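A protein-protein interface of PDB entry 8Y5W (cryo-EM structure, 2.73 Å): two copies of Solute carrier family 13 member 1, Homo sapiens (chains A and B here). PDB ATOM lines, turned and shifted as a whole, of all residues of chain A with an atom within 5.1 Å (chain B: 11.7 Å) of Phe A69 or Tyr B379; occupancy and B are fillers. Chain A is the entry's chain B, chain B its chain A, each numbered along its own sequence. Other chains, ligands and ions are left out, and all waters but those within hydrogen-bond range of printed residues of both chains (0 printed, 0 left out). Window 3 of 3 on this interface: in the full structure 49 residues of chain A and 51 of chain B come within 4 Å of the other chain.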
ATOM      1  N   PRO A  27       5.655  25.208   8.551  1.00  0.00           N
ATOM      2  CA  PRO A  27       5.559  25.464   9.999  1.00  0.00           C
ATOM      3  C   PRO A  27       6.689  26.315  10.548  1.00  0.00           C
ATOM      4  O   PRO A  27       6.453  27.108  11.469  1.00  0.00           O
ATOM      5  CB  PRO A  27       5.574  24.057  10.614  1.00  0.00           C
ATOM      6  CG  PRO A  27       5.214  23.149   9.513  1.00  0.00           C
ATOM      7  CD  PRO A  27       5.775  23.764   8.282  1.00  0.00           C
ATOM      8  N   GLU A  36       1.164  25.551  11.190  1.00  0.00           N
ATOM      9  CA  GLU A  36       1.372  24.186  11.659  1.00  0.00           C
ATOM     10  C   GLU A  36       0.166  23.298  11.380  1.00  0.00           C
ATOM     11  O   GLU A  36       0.322  22.186  10.858  1.00  0.00           O
ATOM     12  CB  GLU A  36       1.685  24.199  13.155  1.00  0.00           C
ATOM     13  CG  GLU A  36       2.920  25.005  13.506  1.00  0.00           C
ATOM     14  CD  GLU A  36       3.109  25.164  14.999  1.00  0.00           C
ATOM     15  OE1 GLU A  36       2.194  24.783  15.758  1.00  0.00           O
ATOM     16  OE2 GLU A  36       4.171  25.674  15.414  1.00  0.00           O
ATOM     17  N   TYR A  39      -0.031  22.780   7.685  1.00  0.00           N
ATOM     18  CA  TYR A  39       0.910  21.738   7.285  1.00  0.00           C
ATOM     19  C   TYR A  39       0.361  20.351   7.587  1.00  0.00           C
ATOM     20  O   TYR A  39       0.456  19.443   6.751  1.00  0.00           O
ATOM     21  CB  TYR A  39       2.244  21.965   7.998  1.00  0.00           C
ATOM     22  CG  TYR A  39       3.219  20.813   7.933  1.00  0.00           C
ATOM     23  CD1 TYR A  39       3.909  20.528   6.767  1.00  0.00           C
ATOM     24  CD2 TYR A  39       3.472  20.030   9.047  1.00  0.00           C
ATOM     25  CE1 TYR A  39       4.808  19.484   6.706  1.00  0.00           C
ATOM     26  CE2 TYR A  39       4.373  18.986   8.995  1.00  0.00           C
ATOM     27  CZ  TYR A  39       5.036  18.717   7.822  1.00  0.00           C
ATOM     28  OH  TYR A  39       5.932  17.676   7.762  1.00  0.00           O
ATOM     29  N   THR A  40      -0.221  20.174   8.774  1.00  0.00           N
ATOM     30  CA  THR A  40      -0.826  18.891   9.122  1.00  0.00           C
ATOM     31  C   THR A  40      -1.959  18.539   8.165  1.00  0.00           C
ATOM     32  O   THR A  40      -2.051  17.400   7.690  1.00  0.00           O
ATOM     33  CB  THR A  40      -1.339  18.926  10.562  1.00  0.00           C
ATOM     34  OG1 THR A  40      -0.274  19.297  11.443  1.00  0.00           O
ATOM     35  CG2 THR A  40      -1.878  17.564  10.970  1.00  0.00           C
ATOM     36  N   MET A  65       0.733  14.764  15.188  1.00  0.00           N
ATOM     37  CA  MET A  65       1.196  16.071  14.748  1.00  0.00           C
ATOM     38  C   MET A  65       0.598  17.197  15.582  1.00  0.00           C
ATOM     39  O   MET A  65       1.313  18.126  15.970  1.00  0.00           O
ATOM     40  CB  MET A  65       0.867  16.244  13.267  1.00  0.00           C
ATOM     41  CG  MET A  65       1.650  15.285  12.383  1.00  0.00           C
ATOM     42  SD  MET A  65       1.237  15.391  10.637  1.00  0.00           S
ATOM     43  CE  MET A  65       1.950  16.976  10.242  1.00  0.00           C
ATOM     44  N   LEU A  66      -0.701  17.132  15.869  1.00  0.00           N
ATOM     45  CA  LEU A  66      -1.328  18.185  16.663  1.00  0.00           C
ATOM     46  C   LEU A  66      -0.757  18.301  18.074  1.00  0.00           C
ATOM     47  O   LEU A  66      -0.460  19.433  18.491  1.00  0.00           O
ATOM     48  CB  LEU A  66      -2.848  17.977  16.701  1.00  0.00           C
ATOM     49  CG  LEU A  66      -3.570  17.940  15.352  1.00  0.00           C
ATOM     50  CD1 LEU A  66      -5.030  17.563  15.531  1.00  0.00           C
ATOM     51  CD2 LEU A  66      -3.440  19.270  14.633  1.00  0.00           C
ATOM     52  N   PRO A  67      -0.598  17.225  18.858  1.00  0.00           N
ATOM     53  CA  PRO A  67       0.031  17.390  20.179  1.00  0.00           C
ATOM     54  C   PRO A  67       1.460  17.900  20.117  1.00  0.00           C
ATOM     55  O   PRO A  67       1.862  18.678  20.992  1.00  0.00           O
ATOM     56  CB  PRO A  67      -0.037  15.979  20.780  1.00  0.00           C
ATOM     57  CG  PRO A  67      -1.149  15.321  20.060  1.00  0.00           C
ATOM     58  CD  PRO A  67      -1.065  15.840  18.663  1.00  0.00           C
ATOM     59  N   MET A  68       2.241  17.492  19.115  1.00  0.00           N
ATOM     60  CA  MET A  68       3.635  17.917  19.042  1.00  0.00           C
ATOM     61  C   MET A  68       3.773  19.369  18.604  1.00  0.00           C
ATOM     62  O   MET A  68       4.677  20.067  19.072  1.00  0.00           O
ATOM     63  CB  MET A  68       4.417  17.005  18.098  1.00  0.00           C
ATOM     64  CG  MET A  68       4.699  15.628  18.673  1.00  0.00           C
ATOM     65  SD  MET A  68       6.017  14.758  17.811  1.00  0.00           S
ATOM     66  CE  MET A  68       5.070  13.605  16.822  1.00  0.00           C
ATOM     67  N   PHE A  69       2.899  19.838  17.715  1.00  0.00           N
ATOM     68  CA  PHE A  69       2.905  21.242  17.327  1.00  0.00           C
ATOM     69  C   PHE A  69       2.365  22.157  18.416  1.00  0.00           C
ATOM     70  O   PHE A  69       2.484  23.380  18.288  1.00  0.00           O
ATOM     71  CB  PHE A  69       2.093  21.445  16.045  1.00  0.00           C
ATOM     72  CG  PHE A  69       2.846  21.114  14.790  1.00  0.00           C
ATOM     73  CD1 PHE A  69       4.025  21.770  14.482  1.00  0.00           C
ATOM     74  CD2 PHE A  69       2.367  20.163  13.907  1.00  0.00           C
ATOM     75  CE1 PHE A  69       4.715  21.474  13.327  1.00  0.00           C
ATOM     76  CE2 PHE A  69       3.055  19.863  12.752  1.00  0.00           C
ATOM     77  CZ  PHE A  69       4.230  20.519  12.462  1.00  0.00           C
ATOM     78  N   GLY A  70       1.782  21.603  19.475  1.00  0.00           N
ATOM     79  CA  GLY A  70       1.209  22.417  20.527  1.00  0.00           C
ATOM     80  C   GLY A  70      -0.168  22.954  20.228  1.00  0.00           C
ATOM     81  O   GLY A  70      -0.640  23.845  20.938  1.00  0.00           O
ATOM     82  N   ILE A  71      -0.826  22.440  19.191  1.00  0.00           N
ATOM     83  CA  ILE A  71      -2.148  22.931  18.819  1.00  0.00           C
ATOM     84  C   ILE A  71      -3.184  22.541  19.865  1.00  0.00           C
ATOM     85  O   ILE A  71      -4.003  23.365  20.287  1.00  0.00           O
ATOM     86  CB  ILE A  71      -2.521  22.412  17.418  1.00  0.00           C
ATOM     87  CG1 ILE A  71      -1.657  23.103  16.361  1.00  0.00           C
ATOM     88  CG2 ILE A  71      -4.000  22.619  17.140  1.00  0.00           C
ATOM     89  CD1 ILE A  71      -1.605  22.378  15.044  1.00  0.00           C
ATOM     90  N   ASP B  84      -6.030   8.634  25.815  1.00  0.00           N
ATOM     91  CA  ASP B  84      -4.625   8.350  25.543  1.00  0.00           C
ATOM     92  C   ASP B  84      -4.290   6.880  25.737  1.00  0.00           C
ATOM     93  O   ASP B  84      -3.336   6.385  25.123  1.00  0.00           O
ATOM     94  CB  ASP B  84      -3.729   9.206  26.437  1.00  0.00           C
ATOM     95  CG  ASP B  84      -3.207  10.436  25.730  1.00  0.00           C
ATOM     96  OD1 ASP B  84      -3.510  10.605  24.532  1.00  0.00           O
ATOM     97  OD2 ASP B  84      -2.489  11.230  26.372  1.00  0.00           O
ATOM     98  N   ARG B 277       2.148  16.263  40.354  1.00  0.00           N
ATOM     99  CA  ARG B 277       3.154  15.911  39.358  1.00  0.00           C
ATOM    100  C   ARG B 277       4.069  14.800  39.864  1.00  0.00           C
ATOM    101  O   ARG B 277       5.284  14.828  39.656  1.00  0.00           O
ATOM    102  CB  ARG B 277       3.976  17.135  38.964  1.00  0.00           C
ATOM    103  CG  ARG B 277       3.292  18.060  37.970  1.00  0.00           C
ATOM    104  CD  ARG B 277       2.448  19.108  38.675  1.00  0.00           C
ATOM    105  NE  ARG B 277       2.043  20.179  37.771  1.00  0.00           N
ATOM    106  CZ  ARG B 277       0.923  20.177  37.062  1.00  0.00           C
ATOM    107  NH1 ARG B 277       0.071  19.168  37.120  1.00  0.00           N
ATOM    108  NH2 ARG B 277       0.653  21.214  36.274  1.00  0.00           N
ATOM    109  N   ARG B 364      11.306  10.836  28.569  1.00  0.00           N
ATOM    110  CA  ARG B 364      10.355  11.845  29.010  1.00  0.00           C
ATOM    111  C   ARG B 364      10.522  12.041  30.509  1.00  0.00           C
ATOM    112  O   ARG B 364      10.713  11.067  31.244  1.00  0.00           O
ATOM    113  CB  ARG B 364       8.927  11.428  28.667  1.00  0.00           C
ATOM    114  CG  ARG B 364       7.930  12.571  28.683  1.00  0.00           C
ATOM    115  CD  ARG B 364       6.536  12.103  28.310  1.00  0.00           C
ATOM    116  NE  ARG B 364       5.948  11.266  29.348  1.00  0.00           N
ATOM    117  CZ  ARG B 364       5.336  11.733  30.427  1.00  0.00           C
ATOM    118  NH1 ARG B 364       5.208  13.032  30.641  1.00  0.00           N
ATOM    119  NH2 ARG B 364       4.841  10.874  31.315  1.00  0.00           N
ATOM    120  N   ASP B 365      10.435  13.298  30.960  1.00  0.00           N
ATOM    121  CA  ASP B 365      11.033  13.763  32.211  1.00  0.00           C
ATOM    122  C   ASP B 365      10.884  12.766  33.354  1.00  0.00           C
ATOM    123  O   ASP B 365       9.771  12.521  33.837  1.00  0.00           O
ATOM    124  CB  ASP B 365      10.425  15.108  32.616  1.00  0.00           C
ATOM    125  CG  ASP B 365       8.912  15.115  32.531  1.00  0.00           C
ATOM    126  OD1 ASP B 365       8.339  14.137  32.009  1.00  0.00           O
ATOM    127  OD2 ASP B 365       8.296  16.099  32.989  1.00  0.00           O
ATOM    128  N   TRP B 372      13.427  15.015  27.031  1.00  0.00           N
ATOM    129  CA  TRP B 372      12.895  15.679  25.852  1.00  0.00           C
ATOM    130  C   TRP B 372      11.600  16.433  26.108  1.00  0.00           C
ATOM    131  O   TRP B 372      11.072  17.052  25.178  1.00  0.00           O
ATOM    132  CB  TRP B 372      12.691  14.676  24.701  1.00  0.00           C
ATOM    133  CG  TRP B 372      11.733  13.556  24.980  1.00  0.00           C
ATOM    134  CD1 TRP B 372      12.047  12.299  25.402  1.00  0.00           C
ATOM    135  CD2 TRP B 372      10.308  13.580  24.820  1.00  0.00           C
ATOM    136  NE1 TRP B 372      10.909  11.544  25.530  1.00  0.00           N
ATOM    137  CE2 TRP B 372       9.828  12.307  25.178  1.00  0.00           C
ATOM    138  CE3 TRP B 372       9.394  14.556  24.416  1.00  0.00           C
ATOM    139  CZ2 TRP B 372       8.474  11.986  25.147  1.00  0.00           C
ATOM    140  CZ3 TRP B 372       8.051  14.235  24.386  1.00  0.00           C
ATOM    141  CH2 TRP B 372       7.604  12.962  24.750  1.00  0.00           C
ATOM    142  N   SER B 373      11.072  16.407  27.333  1.00  0.00           N
ATOM    143  CA  SER B 373       9.957  17.284  27.664  1.00  0.00           C
ATOM    144  C   SER B 373      10.383  18.745  27.651  1.00  0.00           C
ATOM    145  O   SER B 373       9.565  19.627  27.364  1.00  0.00           O
ATOM    146  CB  SER B 373       9.378  16.913  29.027  1.00  0.00           C
ATOM    147  OG  SER B 373       8.851  15.599  29.013  1.00  0.00           O
ATOM    148  N   ALA B 374      11.653  19.019  27.959  1.00  0.00           N
ATOM    149  CA  ALA B 374      12.168  20.380  27.893  1.00  0.00           C
ATOM    150  C   ALA B 374      12.257  20.895  26.463  1.00  0.00           C
ATOM    151  O   ALA B 374      12.297  22.113  26.259  1.00  0.00           O
ATOM    152  CB  ALA B 374      13.540  20.457  28.561  1.00  0.00           C
ATOM    153  N   LEU B 375      12.299  19.999  25.474  1.00  0.00           N
ATOM    154  CA  LEU B 375      12.240  20.438  24.084  1.00  0.00           C
ATOM    155  C   LEU B 375      10.909  21.106  23.774  1.00  0.00           C
ATOM    156  O   LEU B 375      10.866  22.087  23.024  1.00  0.00           O
ATOM    157  CB  LEU B 375      12.471  19.255  23.145  1.00  0.00           C
ATOM    158  CG  LEU B 375      13.849  18.597  23.190  1.00  0.00           C
ATOM    159  CD1 LEU B 375      13.873  17.359  22.310  1.00  0.00           C
ATOM    160  CD2 LEU B 375      14.929  19.579  22.769  1.00  0.00           C
ATOM    161  N   PHE B 376       9.821  20.591  24.338  1.00  0.00           N
ATOM    162  CA  PHE B 376       8.489  21.162  24.186  1.00  0.00           C
ATOM    163  C   PHE B 376       8.071  21.919  25.442  1.00  0.00           C
ATOM    164  O   PHE B 376       6.910  21.880  25.850  1.00  0.00           O
ATOM    165  CB  PHE B 376       7.468  20.075  23.860  1.00  0.00           C
ATOM    166  CG  PHE B 376       7.842  19.221  22.683  1.00  0.00           C
ATOM    167  CD1 PHE B 376       7.719  19.704  21.392  1.00  0.00           C
ATOM    168  CD2 PHE B 376       8.310  17.932  22.868  1.00  0.00           C
ATOM    169  CE1 PHE B 376       8.059  18.917  20.309  1.00  0.00           C
ATOM    170  CE2 PHE B 376       8.653  17.142  21.789  1.00  0.00           C
ATOM    171  CZ  PHE B 376       8.526  17.636  20.509  1.00  0.00           C
ATOM    172  N   SER B 377       9.013  22.617  26.073  1.00  0.00           N
ATOM    173  CA  SER B 377       8.736  23.295  27.340  1.00  0.00           C
ATOM    174  C   SER B 377       8.049  24.639  27.120  1.00  0.00           C
ATOM    175  O   SER B 377       8.434  25.669  27.671  1.00  0.00           O
ATOM    176  CB  SER B 377      10.028  23.464  28.129  1.00  0.00           C
ATOM    177  OG  SER B 377       9.792  24.125  29.360  1.00  0.00           O
ATOM    178  N   GLU B 378       7.008  24.615  26.294  1.00  0.00           N
ATOM    179  CA  GLU B 378       6.052  25.707  26.178  1.00  0.00           C
ATOM    180  C   GLU B 378       4.618  25.225  26.054  1.00  0.00           C
ATOM    181  O   GLU B 378       3.698  26.039  26.199  1.00  0.00           O
ATOM    182  CB  GLU B 378       6.390  26.607  24.979  1.00  0.00           C
ATOM    183  CG  GLU B 378       6.355  25.904  23.636  1.00  0.00           C
ATOM    184  CD  GLU B 378       7.653  25.191  23.311  1.00  0.00           C
ATOM    185  OE1 GLU B 378       7.635  24.282  22.456  1.00  0.00           O
ATOM    186  OE2 GLU B 378       8.692  25.544  23.907  1.00  0.00           O
ATOM    187  N   TYR B 379       4.398  23.934  25.793  1.00  0.00           N
ATOM    188  CA  TYR B 379       3.079  23.309  25.771  1.00  0.00           C
ATOM    189  C   TYR B 379       3.151  22.099  26.695  1.00  0.00           C
ATOM    190  O   TYR B 379       3.237  20.953  26.229  1.00  0.00           O
ATOM    191  CB  TYR B 379       2.671  22.898  24.358  1.00  0.00           C
ATOM    192  CG  TYR B 379       3.005  23.913  23.291  1.00  0.00           C
ATOM    193  CD1 TYR B 379       2.396  25.159  23.274  1.00  0.00           C
ATOM    194  CD2 TYR B 379       3.929  23.622  22.295  1.00  0.00           C
ATOM    195  CE1 TYR B 379       2.698  26.087  22.298  1.00  0.00           C
ATOM    196  CE2 TYR B 379       4.234  24.542  21.314  1.00  0.00           C
ATOM    197  CZ  TYR B 379       3.618  25.774  21.322  1.00  0.00           C
ATOM    198  OH  TYR B 379       3.922  26.697  20.347  1.00  0.00           O
ATOM    199  N   PRO B 380       3.128  22.315  28.011  1.00  0.00           N
ATOM    200  CA  PRO B 380       3.350  21.208  28.955  1.00  0.00           C
ATOM    201  C   PRO B 380       2.191  20.222  28.937  1.00  0.00           C
ATOM    202  O   PRO B 380       1.025  20.610  29.030  1.00  0.00           O
ATOM    203  CB  PRO B 380       3.470  21.917  30.309  1.00  0.00           C
ATOM    204  CG  PRO B 380       2.707  23.182  30.135  1.00  0.00           C
ATOM    205  CD  PRO B 380       2.878  23.592  28.700  1.00  0.00           C
ATOM    206  N   GLY B 381       2.522  18.939  28.818  1.00  0.00           N
ATOM    207  CA  GLY B 381       1.520  17.896  28.873  1.00  0.00           C
ATOM    208  C   GLY B 381       0.812  17.603  27.572  1.00  0.00           C
ATOM    209  O   GLY B 381      -0.121  16.795  27.561  1.00  0.00           O
ATOM    210  N   PHE B 382       1.224  18.229  26.468  1.00  0.00           N
ATOM    211  CA  PHE B 382       0.575  17.949  25.191  1.00  0.00           C
ATOM    212  C   PHE B 382       1.077  16.636  24.602  1.00  0.00           C
ATOM    213  O   PHE B 382       0.282  15.760  24.252  1.00  0.00           O
ATOM    214  CB  PHE B 382       0.798  19.096  24.202  1.00  0.00           C
ATOM    215  CG  PHE B 382       0.011  20.344  24.512  1.00  0.00           C
ATOM    216  CD1 PHE B 382      -0.472  20.594  25.784  1.00  0.00           C
ATOM    217  CD2 PHE B 382      -0.271  21.256  23.510  1.00  0.00           C
ATOM    218  CE1 PHE B 382      -1.190  21.740  26.056  1.00  0.00           C
ATOM    219  CE2 PHE B 382      -0.994  22.399  23.776  1.00  0.00           C
ATOM    220  CZ  PHE B 382      -1.454  22.641  25.049  1.00  0.00           C
ATOM    221  N   ALA B 383       2.394  16.486  24.486  1.00  0.00           N
ATOM    222  CA  ALA B 383       2.979  15.236  24.026  1.00  0.00           C
ATOM    223  C   ALA B 383       3.191  14.305  25.211  1.00  0.00           C
ATOM    224  O   ALA B 383       3.830  14.679  26.199  1.00  0.00           O
ATOM    225  CB  ALA B 383       4.301  15.496  23.306  1.00  0.00           C
ATOM    226  N   THR B 384       2.659  13.094  25.112  1.00  0.00           N
ATOM    227  CA  THR B 384       2.682  12.125  26.198  1.00  0.00           C
ATOM    228  C   THR B 384       3.323  10.825  25.717  1.00  0.00           C
ATOM    229  O   THR B 384       3.904  10.757  24.630  1.00  0.00           O
ATOM    230  CB  THR B 384       1.269  11.884  26.735  1.00  0.00           C
ATOM    231  OG1 THR B 384       0.447  11.344  25.694  1.00  0.00           O
ATOM    232  CG2 THR B 384       0.654  13.182  27.231  1.00  0.00           C
ATOM    233  N   ASP B 385       3.226   9.788  26.551  1.00  0.00           N
ATOM    234  CA  ASP B 385       3.729   8.473  26.171  1.00  0.00           C
ATOM    235  C   ASP B 385       2.939   7.869  25.020  1.00  0.00           C
ATOM    236  O   ASP B 385       3.498   7.091  24.238  1.00  0.00           O
ATOM    237  CB  ASP B 385       3.698   7.533  27.376  1.00  0.00           C
ATOM    238  CG  ASP B 385       4.769   7.861  28.396  1.00  0.00           C
ATOM    239  OD1 ASP B 385       5.905   8.182  27.989  1.00  0.00           O
ATOM    240  OD2 ASP B 385       4.475   7.797  29.607  1.00  0.00           O
ATOM    241  N   THR B 387       1.906   9.579  22.493  1.00  0.00           N
ATOM    242  CA  THR B 387       2.540  10.157  21.313  1.00  0.00           C
ATOM    243  C   THR B 387       3.776   9.362  20.909  1.00  0.00           C
ATOM    244  O   THR B 387       3.987   9.095  19.722  1.00  0.00           O
ATOM    245  CB  THR B 387       2.901  11.620  21.576  1.00  0.00           C
ATOM    246  OG1 THR B 387       1.738  12.326  22.022  1.00  0.00           O
ATOM    247  CG2 THR B 387       3.428  12.279  20.314  1.00  0.00           C
ATOM    248  N   LEU B 391       4.166   7.365  17.403  1.00  0.00           N
ATOM    249  CA  LEU B 391       5.271   7.688  16.508  1.00  0.00           C
ATOM    250  C   LEU B 391       6.076   6.446  16.158  1.00  0.00           C
ATOM    251  O   LEU B 391       6.450   6.249  14.996  1.00  0.00           O
ATOM    252  CB  LEU B 391       6.168   8.748  17.144  1.00  0.00           C
ATOM    253  CG  LEU B 391       7.377   9.212  16.331  1.00  0.00           C
ATOM    254  CD1 LEU B 391       6.935   9.904  15.055  1.00  0.00           C
ATOM    255  CD2 LEU B 391       8.257  10.128  17.162  1.00  0.00           C
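No position is printed for both chains.
Of the 6 pairs that touch across the chains among the printed residues, none has its exchanged pair printed and touching as well.
Of the 11 printed residues of chain A, 4 touch a printed residue of chain B.
Hydrophobic or aromatic side chains of chain A that line the printed part of chain B: Pro A67 and Met A68.
Among the printed residues, 6 pairs touch across the chains.
OG1 of Thr B387 sits at hydrogen-bond distance from N of Thr B384, at 3.3 Å.
No residue of chain B comes within 4 Å of Pro A27.
Glu A36 touches none of the printed residues of chain B.
No residue of chain B comes within 4 Å of Tyr A39.
No residue of chain B comes within 4 Å of Thr A40.
Of chain B, only Phe B382 (3.4 Å) comes within 4 Å of Pro A67.
Of chain B, only Tyr B379 comes within 4 Å of Phe A69.
Of the printed residues of chain B, Gly A70 touches Tyr B379 (3.5 Å) and Phe B382 (3.2 Å).
No residue of chain B comes within 4 Å of Ile A71.
Arg B277 touches none of the printed residues of chain A.
Printed residues of chain A within 4 Å of Phe B376: Met A68.
Gly B381 touches none of the printed residues of chain A.
Of the printed residues of chain A, Phe B382 touches Pro A67 (3.4 Å) and Gly A70 (3.2 Å).
Of the printed residues of chain A, Thr B387 touches Met A68 (3.9 Å).
The nearest residue of chain B that does not touch Phe A69 is Phe B382 (5.8 Å).
The nearest residue of chain A that does not touch Tyr B379 is Met A68 (4.9 Å).
The nearest printed residue of chain A that does not touch Thr B387 is Pro A67 (4.2 Å).
CB of Phe B382 touches O of Pro A67 (3.4 Å).
CE1 of Phe B376 touches O of Met A68 (3.8 Å).
Met A68 touches Thr B387 (CG to CG2, 3.9 Å).
Tyr B379 touches Phe A69 (CE2 to O, 3.7 Å).
Gly A70 touches Tyr B379 (CA to CD2, 3.5 Å).
Phe B382 touches Gly A70 (CE2 to O, 3.2 Å).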
